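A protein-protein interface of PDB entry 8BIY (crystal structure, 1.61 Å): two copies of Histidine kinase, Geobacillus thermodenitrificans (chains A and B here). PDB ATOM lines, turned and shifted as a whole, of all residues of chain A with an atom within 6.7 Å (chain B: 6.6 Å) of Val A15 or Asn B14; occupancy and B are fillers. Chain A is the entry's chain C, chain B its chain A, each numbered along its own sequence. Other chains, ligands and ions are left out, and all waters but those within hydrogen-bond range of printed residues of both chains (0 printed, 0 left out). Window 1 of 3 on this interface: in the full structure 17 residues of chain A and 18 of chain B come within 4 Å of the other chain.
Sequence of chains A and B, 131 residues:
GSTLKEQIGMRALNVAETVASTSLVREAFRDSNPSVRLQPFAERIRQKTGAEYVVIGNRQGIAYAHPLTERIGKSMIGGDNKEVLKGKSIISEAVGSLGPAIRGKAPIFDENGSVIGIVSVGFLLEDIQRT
Arg B11 touches its own counterpart, Arg A11. Arg A11 touches Asn B14, and with the chains exchanged Asn A14 touches Arg B11. Glu A17 touches Thr B49, but with the chains exchanged Thr A49 does not touch Glu B17 (4.05 Å). Thr A18 touches Thr B49, and with the chains exchanged Thr A49 touches Thr B18. 12 positions are printed for both chains. Of the 16 pairs that touch across the chains among the printed residues, 12 have their exchanged pair printed and touching as well.
Among the printed residues, pairs that only touch across the chains: Met A10 with Arg B11 (3.3 Å), Arg A11 with Met B10 (3.6 Å), Arg A11 with Arg B11 (3.6 Å), Asn A14 with Val B15 (3.7 Å), Val A15 with Asn B14 (3.7 Å), Glu A17 with Thr B49 (3.9 Å), Thr A18 with Thr B18 (3.5 Å), Thr A18 with Thr B49 (3.7 Å), Ile A45 with Thr B18 (3.8 Å), Thr A49 with Thr B18 (3.6 Å) and Phe A123 with Asn B14 (3.5 Å).
The backbone carbonyl oxygen (O) of Met B10 sits close to the side-chain amide nitrogen (ND2) of Asn B14, at 3.5 Å. The guanidinium group (NH2) of Arg B11 sits at hydrogen-bond distance from the backbone carbonyl oxygen (O) of Thr B49, 3.0 Å away. O of Asn B14 sits at hydrogen-bond distance from OG1 of Thr B18, 2.7 Å away. The guanidinium group (NH2) of Arg A11 is in hydrogen-bond range of the backbone carbonyl oxygen (O) of Thr A49 (3.0 Å). ND2 of Asn A14 lies within hydrogen-bond range of OE1 of Glu A17. OG1 of Thr A49 sits at hydrogen-bond distance from O of Ile A45 (2.9 Å).
Along chain A the printed residues that touch a printed residue of chain B span positions 10 to 123.
NE of Arg B11 is in hydrogen-bond range of OD1 of Asn A14 (2.6 Å). The guanidinium group (NE) of Arg A11 lies within hydrogen-bond range of the side-chain amide oxygen (OD1) of Asn B14 (2.8 Å). ND2 of Asn B14 sits at hydrogen-bond distance from O of Thr A49 (3.3 Å). The side-chain amide nitrogen of Asn A14 is in hydrogen-bond range of the backbone carbonyl oxygen of Thr B49, at 3.4 Å. O of Lys A48 sits close to OE1 of Glu B17 (3.2 Å).
Printed residues of chain B within 4 Å of Asn A14: Arg B11, Val B15 and Thr B49. Of the printed residues of chain B, Val A15 touches Asn B14 (3.7 Å). Of the printed residues of chain B, Ile A45 touches Thr B18 (3.8 Å). Gly B9 touches none of the printed residues of chain A. Ala B12 touches none of the printed residues of chain A. Of chain A, only Arg A11, Val A15, Thr A49 and Phe A123 come within 4 Å of Asn B14. The nearest residue of chain B that does not touch Val A15 is Thr B18 (4.2 Å). The nearest residue of chain A that does not touch Asn B14 is Lys A48 (4.7 Å). The nearest printed residue of chain A that does not touch Arg B11 is Val A15 (6.2 Å).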
ATOM      1  N   MET A  10      -1.611   8.365 -26.070  1.00  0.00           N
ATOM      2  CA  MET A  10      -2.449   8.372 -24.878  1.00  0.00           C
ATOM      3  C   MET A  10      -2.958   6.974 -24.553  1.00  0.00           C
ATOM      4  O   MET A  10      -3.091   6.628 -23.372  1.00  0.00           O
ATOM      5  CB  MET A  10      -3.618   9.347 -25.051  1.00  0.00           C
ATOM      6  CG  MET A  10      -3.220  10.809 -25.131  1.00  0.00           C
ATOM      7  SD  MET A  10      -2.207  11.313 -23.735  1.00  0.00           S
ATOM      8  CE  MET A  10      -3.308  10.991 -22.359  1.00  0.00           C
ATOM      9  N   ARG A  11      -3.266   6.165 -25.580  1.00  0.00           N
ATOM     10  CA  ARG A  11      -3.531   4.742 -25.365  1.00  0.00           C
ATOM     11  C   ARG A  11      -2.388   4.091 -24.601  1.00  0.00           C
ATOM     12  O   ARG A  11      -2.604   3.437 -23.573  1.00  0.00           O
ATOM     13  CB  ARG A  11      -3.714   4.009 -26.694  1.00  0.00           C
ATOM     14  CG  ARG A  11      -5.122   3.825 -27.175  1.00  0.00           C
ATOM     15  CD  ARG A  11      -5.105   3.049 -28.482  1.00  0.00           C
ATOM     16  NE  ARG A  11      -5.033   1.606 -28.274  1.00  0.00           N
ATOM     17  CZ  ARG A  11      -5.106   0.714 -29.252  1.00  0.00           C
ATOM     18  NH1 ARG A  11      -5.127   1.084 -30.524  1.00  0.00           N
ATOM     19  NH2 ARG A  11      -5.161  -0.580 -28.951  1.00  0.00           N
ATOM     20  N   ALA A  12      -1.162   4.248 -25.112  1.00  0.00           N
ATOM     21  CA  ALA A  12       0.010   3.641 -24.488  1.00  0.00           C
ATOM     22  C   ALA A  12       0.169   4.115 -23.049  1.00  0.00           C
ATOM     23  O   ALA A  12       0.396   3.311 -22.134  1.00  0.00           O
ATOM     24  CB  ALA A  12       1.264   3.973 -25.316  1.00  0.00           C
ATOM     25  N   LEU A  13       0.043   5.423 -22.826  1.00  0.00           N
ATOM     26  CA  LEU A  13       0.256   5.959 -21.490  1.00  0.00           C
ATOM     27  C   LEU A  13      -0.841   5.504 -20.527  1.00  0.00           C
ATOM     28  O   LEU A  13      -0.555   5.153 -19.381  1.00  0.00           O
ATOM     29  CB  LEU A  13       0.314   7.481 -21.541  1.00  0.00           C
ATOM     30  CG  LEU A  13       0.622   8.159 -20.211  1.00  0.00           C
ATOM     31  CD1 LEU A  13       1.923   7.616 -19.617  1.00  0.00           C
ATOM     32  CD2 LEU A  13       0.672   9.666 -20.394  1.00  0.00           C
ATOM     33  N   ASN A  14      -2.100   5.497 -20.971  1.00  0.00           N
ATOM     34  CA  ASN A  14      -3.176   5.055 -20.087  1.00  0.00           C
ATOM     35  C   ASN A  14      -3.020   3.590 -19.683  1.00  0.00           C
ATOM     36  O   ASN A  14      -3.286   3.230 -18.529  1.00  0.00           O
ATOM     37  CB  ASN A  14      -4.522   5.266 -20.752  1.00  0.00           C
ATOM     38  CG  ASN A  14      -4.969   6.713 -20.748  1.00  0.00           C
ATOM     39  OD1 ASN A  14      -6.016   7.018 -21.287  1.00  0.00           O
ATOM     40  ND2 ASN A  14      -4.203   7.594 -20.119  1.00  0.00           N
ATOM     41  N   VAL A  15      -2.589   2.729 -20.606  1.00  0.00           N
ATOM     42  CA  VAL A  15      -2.330   1.337 -20.228  1.00  0.00           C
ATOM     43  C   VAL A  15      -1.184   1.275 -19.224  1.00  0.00           C
ATOM     44  O   VAL A  15      -1.260   0.566 -18.217  1.00  0.00           O
ATOM     45  CB  VAL A  15      -2.044   0.469 -21.468  1.00  0.00           C
ATOM     46  CG1 VAL A  15      -1.699  -0.992 -21.068  1.00  0.00           C
ATOM     47  CG2 VAL A  15      -3.268   0.459 -22.434  1.00  0.00           C
ATOM     48  N   ALA A  16      -0.097   2.018 -19.480  1.00  0.00           N
ATOM     49  CA  ALA A  16       1.041   1.978 -18.563  1.00  0.00           C
ATOM     50  C   ALA A  16       0.654   2.462 -17.172  1.00  0.00           C
ATOM     51  O   ALA A  16       1.026   1.847 -16.164  1.00  0.00           O
ATOM     52  CB  ALA A  16       2.200   2.823 -19.117  1.00  0.00           C
ATOM     53  N   GLU A  17      -0.095   3.566 -17.104  1.00  0.00           N
ATOM     54  CA  GLU A  17      -0.525   4.111 -15.821  1.00  0.00           C
ATOM     55  C   GLU A  17      -1.413   3.132 -15.076  1.00  0.00           C
ATOM     56  O   GLU A  17      -1.286   2.982 -13.855  1.00  0.00           O
ATOM     57  CB  GLU A  17      -1.278   5.416 -16.048  1.00  0.00           C
ATOM     58  CG  GLU A  17      -0.401   6.527 -16.560  1.00  0.00           C
ATOM     59  CD  GLU A  17      -1.196   7.755 -16.956  1.00  0.00           C
ATOM     60  OE1 GLU A  17      -2.228   7.605 -17.653  1.00  0.00           O
ATOM     61  OE2 GLU A  17      -0.761   8.872 -16.606  1.00  0.00           O
ATOM     62  N   THR A  18      -2.332   2.472 -15.796  1.00  0.00           N
ATOM     63  CA  THR A  18      -3.212   1.500 -15.153  1.00  0.00           C
ATOM     64  C   THR A  18      -2.424   0.302 -14.631  1.00  0.00           C
ATOM     65  O   THR A  18      -2.636  -0.138 -13.494  1.00  0.00           O
ATOM     66  CB  THR A  18      -4.314   1.058 -16.114  1.00  0.00           C
ATOM     67  OG1 THR A  18      -5.005   2.216 -16.602  1.00  0.00           O
ATOM     68  CG2 THR A  18      -5.328   0.154 -15.398  1.00  0.00           C
ATOM     69  N   VAL A  19      -1.483  -0.214 -15.430  1.00  0.00           N
ATOM     70  CA  VAL A  19      -0.643  -1.320 -14.970  1.00  0.00           C
ATOM     71  C   VAL A  19       0.177  -0.885 -13.757  1.00  0.00           C
ATOM     72  O   VAL A  19       0.274  -1.611 -12.760  1.00  0.00           O
ATOM     73  CB  VAL A  19       0.259  -1.808 -16.119  1.00  0.00           C
ATOM     74  CG1 VAL A  19       1.299  -2.846 -15.611  1.00  0.00           C
ATOM     75  CG2 VAL A  19      -0.571  -2.409 -17.234  1.00  0.00           C
ATOM     76  N   ALA A  20       0.749   0.324 -13.816  1.00  0.00           N
ATOM     77  CA  ALA A  20       1.606   0.809 -12.729  1.00  0.00           C
ATOM     78  C   ALA A  20       0.839   0.971 -11.415  1.00  0.00           C
ATOM     79  O   ALA A  20       1.448   0.951 -10.334  1.00  0.00           O
ATOM     80  CB  ALA A  20       2.255   2.135 -13.118  1.00  0.00           C
ATOM     81  N   ILE A  45      -2.075  -8.320 -20.225  1.00  0.00           N
ATOM     82  CA  ILE A  45      -2.458  -6.966 -20.619  1.00  0.00           C
ATOM     83  C   ILE A  45      -2.013  -6.674 -22.044  1.00  0.00           C
ATOM     84  O   ILE A  45      -2.744  -6.045 -22.818  1.00  0.00           O
ATOM     85  CB  ILE A  45      -1.900  -5.925 -19.631  1.00  0.00           C
ATOM     86  CG1 ILE A  45      -2.467  -6.168 -18.228  1.00  0.00           C
ATOM     87  CG2 ILE A  45      -2.195  -4.490 -20.128  1.00  0.00           C
ATOM     88  CD1 ILE A  45      -4.009  -6.363 -18.230  1.00  0.00           C
ATOM     89  N   ARG A  46      -0.793  -7.096 -22.399  1.00  0.00           N
ATOM     90  CA  ARG A  46      -0.289  -6.869 -23.748  1.00  0.00           C
ATOM     91  C   ARG A  46      -1.207  -7.515 -24.784  1.00  0.00           C
ATOM     92  O   ARG A  46      -1.575  -6.884 -25.781  1.00  0.00           O
ATOM     93  CB  ARG A  46       1.147  -7.401 -23.867  1.00  0.00           C
ATOM     94  CG  ARG A  46       1.834  -7.009 -25.180  1.00  0.00           C
ATOM     95  CD  ARG A  46       3.112  -7.824 -25.367  1.00  0.00           C
ATOM     96  NE  ARG A  46       2.742  -9.183 -25.736  1.00  0.00           N
ATOM     97  CZ  ARG A  46       2.224  -9.537 -26.906  1.00  0.00           C
ATOM     98  NH1 ARG A  46       2.186  -8.695 -27.936  1.00  0.00           N
ATOM     99  NH2 ARG A  46       1.712 -10.762 -27.046  1.00  0.00           N
ATOM    100  N   LYS A  48      -4.479  -8.374 -24.418  1.00  0.00           N
ATOM    101  CA  LYS A  48      -5.843  -7.840 -24.429  1.00  0.00           C
ATOM    102  C   LYS A  48      -5.915  -6.472 -25.093  1.00  0.00           C
ATOM    103  O   LYS A  48      -6.921  -6.137 -25.730  1.00  0.00           O
ATOM    104  CB  LYS A  48      -6.391  -7.723 -23.009  1.00  0.00           C
ATOM    105  CG  LYS A  48      -6.568  -9.038 -22.276  1.00  0.00           C
ATOM    106  CD  LYS A  48      -7.479 -10.009 -22.998  1.00  0.00           C
ATOM    107  CE  LYS A  48      -8.737 -10.301 -22.187  1.00  0.00           C
ATOM    108  NZ  LYS A  48      -9.722 -11.119 -22.952  1.00  0.00           N
ATOM    109  N   THR A  49      -4.883  -5.648 -24.919  1.00  0.00           N
ATOM    110  CA  THR A  49      -4.894  -4.278 -25.412  1.00  0.00           C
ATOM    111  C   THR A  49      -4.364  -4.123 -26.830  1.00  0.00           C
ATOM    112  O   THR A  49      -4.586  -3.068 -27.431  1.00  0.00           O
ATOM    113  CB  THR A  49      -4.073  -3.348 -24.492  1.00  0.00           C
ATOM    114  OG1 THR A  49      -2.679  -3.729 -24.488  1.00  0.00           O
ATOM    115  CG2 THR A  49      -4.626  -3.316 -23.064  1.00  0.00           C
ATOM    116  N   GLY A  50      -3.676  -5.122 -27.377  1.00  0.00           N
ATOM    117  CA  GLY A  50      -3.076  -4.985 -28.694  1.00  0.00           C
ATOM    118  C   GLY A  50      -1.721  -4.315 -28.700  1.00  0.00           C
ATOM    119  O   GLY A  50      -1.229  -3.938 -29.772  1.00  0.00           O
ATOM    120  N   ALA A  51      -1.112  -4.140 -27.541  1.00  0.00           N
ATOM    121  CA  ALA A  51       0.205  -3.524 -27.476  1.00  0.00           C
ATOM    122  C   ALA A  51       1.265  -4.426 -28.092  1.00  0.00           C
ATOM    123  O   ALA A  51       1.145  -5.653 -28.118  1.00  0.00           O
ATOM    124  CB  ALA A  51       0.582  -3.221 -26.026  1.00  0.00           C
ATOM    125  N   VAL A  54       4.431  -4.698 -23.115  1.00  0.00           N
ATOM    126  CA  VAL A  54       4.200  -4.137 -21.786  1.00  0.00           C
ATOM    127  C   VAL A  54       5.416  -4.529 -20.957  1.00  0.00           C
ATOM    128  O   VAL A  54       5.497  -5.651 -20.445  1.00  0.00           O
ATOM    129  CB  VAL A  54       2.905  -4.644 -21.140  1.00  0.00           C
ATOM    130  CG1 VAL A  54       2.755  -4.102 -19.726  1.00  0.00           C
ATOM    131  CG2 VAL A  54       1.686  -4.212 -22.013  1.00  0.00           C
ATOM    132  N   GLY A 104       4.270   4.909 -23.907  1.00  0.00           N
ATOM    133  CA  GLY A 104       4.017   5.646 -22.692  1.00  0.00           C
ATOM    134  C   GLY A 104       4.694   4.996 -21.509  1.00  0.00           C
ATOM    135  O   GLY A 104       4.630   3.776 -21.331  1.00  0.00           O
ATOM    136  N   ALA A 106       5.166   5.069 -17.282  1.00  0.00           N
ATOM    137  CA  ALA A 106       4.597   5.520 -16.022  1.00  0.00           C
ATOM    138  C   ALA A 106       5.441   5.002 -14.869  1.00  0.00           C
ATOM    139  O   ALA A 106       5.960   3.889 -14.933  1.00  0.00           O
ATOM    140  CB  ALA A 106       3.151   5.028 -15.842  1.00  0.00           C
ATOM    141  N   VAL A 119       6.825   1.217 -15.862  1.00  0.00           N
ATOM    142  CA  VAL A 119       6.048   0.493 -16.863  1.00  0.00           C
ATOM    143  C   VAL A 119       6.170   1.236 -18.184  1.00  0.00           C
ATOM    144  O   VAL A 119       5.917   2.446 -18.248  1.00  0.00           O
ATOM    145  CB  VAL A 119       4.574   0.368 -16.453  1.00  0.00           C
ATOM    146  CG1 VAL A 119       3.795  -0.389 -17.550  1.00  0.00           C
ATOM    147  CG2 VAL A 119       4.472  -0.331 -15.125  1.00  0.00           C
ATOM    148  N   VAL A 121       4.804   0.890 -22.107  1.00  0.00           N
ATOM    149  CA  VAL A 121       3.863   0.232 -23.002  1.00  0.00           C
ATOM    150  C   VAL A 121       4.043   0.861 -24.368  1.00  0.00           C
ATOM    151  O   VAL A 121       3.993   2.091 -24.488  1.00  0.00           O
ATOM    152  CB  VAL A 121       2.408   0.423 -22.534  1.00  0.00           C
ATOM    153  CG1 VAL A 121       1.470  -0.135 -23.594  1.00  0.00           C
ATOM    154  CG2 VAL A 121       2.179  -0.239 -21.196  1.00  0.00           C
ATOM    155  N   PHE A 123       2.885   0.804 -28.619  1.00  0.00           N
ATOM    156  CA  PHE A 123       2.011   0.407 -29.717  1.00  0.00           C
ATOM    157  C   PHE A 123       2.681   0.699 -31.054  1.00  0.00           C
ATOM    158  O   PHE A 123       3.268   1.767 -31.239  1.00  0.00           O
ATOM    159  CB  PHE A 123       0.679   1.160 -29.651  1.00  0.00           C
ATOM    160  CG  PHE A 123      -0.269   0.613 -28.616  1.00  0.00           C
ATOM    161  CD1 PHE A 123      -0.189   1.017 -27.291  1.00  0.00           C
ATOM    162  CD2 PHE A 123      -1.222  -0.329 -28.972  1.00  0.00           C
ATOM    163  CE1 PHE A 123      -1.059   0.489 -26.333  1.00  0.00           C
ATOM    164  CE2 PHE A 123      -2.082  -0.857 -28.026  1.00  0.00           C
ATOM    165  CZ  PHE A 123      -2.006  -0.456 -26.714  1.00  0.00           C
ATOM    166  N   GLY B   9     -11.920   5.667 -28.567  1.00  0.00           N
ATOM    167  CA  GLY B   9     -12.667   4.486 -28.163  1.00  0.00           C
ATOM    168  C   GLY B   9     -11.768   3.316 -27.813  1.00  0.00           C
ATOM    169  O   GLY B   9     -12.072   2.536 -26.905  1.00  0.00           O
ATOM    170  N   MET B  10     -10.652   3.169 -28.533  1.00  0.00           N
ATOM    171  CA  MET B  10      -9.692   2.128 -28.171  1.00  0.00           C
ATOM    172  C   MET B  10      -9.008   2.457 -26.855  1.00  0.00           C
ATOM    173  O   MET B  10      -8.698   1.553 -26.071  1.00  0.00           O
ATOM    174  CB  MET B  10      -8.665   1.929 -29.289  1.00  0.00           C
ATOM    175  CG  MET B  10      -9.260   1.353 -30.573  1.00  0.00           C
ATOM    176  SD  MET B  10     -10.022  -0.255 -30.309  1.00  0.00           S
ATOM    177  CE  MET B  10      -8.625  -1.161 -29.642  1.00  0.00           C
ATOM    178  N   ARG B  11      -8.766   3.742 -26.599  1.00  0.00           N
ATOM    179  CA  ARG B  11      -8.229   4.185 -25.315  1.00  0.00           C
ATOM    180  C   ARG B  11      -9.163   3.776 -24.178  1.00  0.00           C
ATOM    181  O   ARG B  11      -8.744   3.173 -23.180  1.00  0.00           O
ATOM    182  CB  ARG B  11      -8.048   5.699 -25.364  1.00  0.00           C
ATOM    183  CG  ARG B  11      -7.425   6.356 -24.172  1.00  0.00           C
ATOM    184  CD  ARG B  11      -7.107   7.827 -24.477  1.00  0.00           C
ATOM    185  NE  ARG B  11      -6.781   8.501 -23.232  1.00  0.00           N
ATOM    186  CZ  ARG B  11      -6.773   9.812 -23.041  1.00  0.00           C
ATOM    187  NH1 ARG B  11      -7.046  10.661 -24.024  1.00  0.00           N
ATOM    188  NH2 ARG B  11      -6.488  10.286 -21.830  1.00  0.00           N
ATOM    189  N   ALA B  12     -10.447   4.082 -24.330  1.00  0.00           N
ATOM    190  CA  ALA B  12     -11.437   3.690 -23.336  1.00  0.00           C
ATOM    191  C   ALA B  12     -11.468   2.180 -23.144  1.00  0.00           C
ATOM    192  O   ALA B  12     -11.493   1.685 -22.009  1.00  0.00           O
ATOM    193  CB  ALA B  12     -12.814   4.207 -23.767  1.00  0.00           C
ATOM    194  N   LEU B  13     -11.504   1.427 -24.246  1.00  0.00           N
ATOM    195  CA  LEU B  13     -11.582  -0.021 -24.145  1.00  0.00           C
ATOM    196  C   LEU B  13     -10.308  -0.599 -23.540  1.00  0.00           C
ATOM    197  O   LEU B  13     -10.378  -1.510 -22.709  1.00  0.00           O
ATOM    198  CB  LEU B  13     -11.853  -0.639 -25.516  1.00  0.00           C
ATOM    199  CG  LEU B  13     -11.992  -2.159 -25.518  1.00  0.00           C
ATOM    200  CD1 LEU B  13     -13.117  -2.584 -24.585  1.00  0.00           C
ATOM    201  CD2 LEU B  13     -12.251  -2.701 -26.927  1.00  0.00           C
ATOM    202  N   ASN B  14      -9.134  -0.081 -23.932  1.00  0.00           N
ATOM    203  CA  ASN B  14      -7.891  -0.589 -23.344  1.00  0.00           C
ATOM    204  C   ASN B  14      -7.854  -0.388 -21.835  1.00  0.00           C
ATOM    205  O   ASN B  14      -7.358  -1.261 -21.107  1.00  0.00           O
ATOM    206  CB  ASN B  14      -6.670   0.089 -23.964  1.00  0.00           C
ATOM    207  CG  ASN B  14      -6.331  -0.433 -25.351  1.00  0.00           C
ATOM    208  OD1 ASN B  14      -5.429   0.087 -25.993  1.00  0.00           O
ATOM    209  ND2 ASN B  14      -7.023  -1.458 -25.802  1.00  0.00           N
ATOM    210  N   VAL B  15      -8.333   0.764 -21.345  1.00  0.00           N
ATOM    211  CA  VAL B  15      -8.373   0.959 -19.893  1.00  0.00           C
ATOM    212  C   VAL B  15      -9.371  -0.007 -19.267  1.00  0.00           C
ATOM    213  O   VAL B  15      -9.093  -0.637 -18.242  1.00  0.00           O
ATOM    214  CB  VAL B  15      -8.702   2.422 -19.537  1.00  0.00           C
ATOM    215  CG1 VAL B  15      -8.867   2.593 -18.032  1.00  0.00           C
ATOM    216  CG2 VAL B  15      -7.603   3.384 -20.042  1.00  0.00           C
ATOM    217  N   ALA B  16     -10.548  -0.158 -19.875  1.00  0.00           N
ATOM    218  CA  ALA B  16     -11.546  -1.065 -19.305  1.00  0.00           C
ATOM    219  C   ALA B  16     -11.038  -2.506 -19.261  1.00  0.00           C
ATOM    220  O   ALA B  16     -11.250  -3.215 -18.269  1.00  0.00           O
ATOM    221  CB  ALA B  16     -12.846  -0.972 -20.114  1.00  0.00           C
ATOM    222  N   GLU B  17     -10.383  -2.951 -20.338  1.00  0.00           N
ATOM    223  CA  GLU B  17      -9.806  -4.291 -20.402  1.00  0.00           C
ATOM    224  C   GLU B  17      -8.727  -4.485 -19.344  1.00  0.00           C
ATOM    225  O   GLU B  17      -8.627  -5.558 -18.739  1.00  0.00           O
ATOM    226  CB  GLU B  17      -9.225  -4.529 -21.803  1.00  0.00           C
ATOM    227  CG  GLU B  17     -10.292  -4.758 -22.867  1.00  0.00           C
ATOM    228  CD  GLU B  17      -9.802  -4.560 -24.300  1.00  0.00           C
ATOM    229  OE1 GLU B  17      -8.813  -3.819 -24.517  1.00  0.00           O
ATOM    230  OE2 GLU B  17     -10.444  -5.120 -25.220  1.00  0.00           O
ATOM    231  N   THR B  18      -7.895  -3.468 -19.120  1.00  0.00           N
ATOM    232  CA  THR B  18      -6.822  -3.609 -18.139  1.00  0.00           C
ATOM    233  C   THR B  18      -7.383  -3.660 -16.719  1.00  0.00           C
ATOM    234  O   THR B  18      -6.987  -4.512 -15.912  1.00  0.00           O
ATOM    235  CB  THR B  18      -5.808  -2.479 -18.320  1.00  0.00           C
ATOM    236  OG1 THR B  18      -5.367  -2.458 -19.687  1.00  0.00           O
ATOM    237  CG2 THR B  18      -4.596  -2.673 -17.395  1.00  0.00           C
ATOM    238  N   VAL B  19      -8.338  -2.781 -16.409  1.00  0.00           N
ATOM    239  CA  VAL B  19      -9.035  -2.832 -15.123  1.00  0.00           C
ATOM    240  C   VAL B  19      -9.701  -4.196 -14.926  1.00  0.00           C
ATOM    241  O   VAL B  19      -9.601  -4.812 -13.857  1.00  0.00           O
ATOM    242  CB  VAL B  19     -10.060  -1.678 -15.042  1.00  0.00           C
ATOM    243  CG1 VAL B  19     -10.946  -1.826 -13.811  1.00  0.00           C
ATOM    244  CG2 VAL B  19      -9.329  -0.356 -14.962  1.00  0.00           C
ATOM    245  N   THR B  49      -5.855   8.333 -15.672  1.00  0.00           N
ATOM    246  CA  THR B  49      -6.026   8.224 -17.115  1.00  0.00           C
ATOM    247  C   THR B  49      -6.736   9.421 -17.740  1.00  0.00           C
ATOM    248  O   THR B  49      -6.741   9.526 -18.962  1.00  0.00           O
ATOM    249  CB  THR B  49      -6.834   6.975 -17.509  1.00  0.00           C
ATOM    250  OG1 THR B  49      -8.146   7.025 -16.930  1.00  0.00           O
ATOM    251  CG2 THR B  49      -6.143   5.673 -17.039  1.00  0.00           C
ATOM    252  N   GLY B 104     -15.808   2.439 -23.580  1.00  0.00           N
ATOM    253  CA  GLY B 104     -15.532   1.048 -23.884  1.00  0.00           C
ATOM    254  C   GLY B 104     -15.931   0.187 -22.706  1.00  0.00           C
ATOM    255  O   GLY B 104     -15.734   0.565 -21.550  1.00  0.00           O
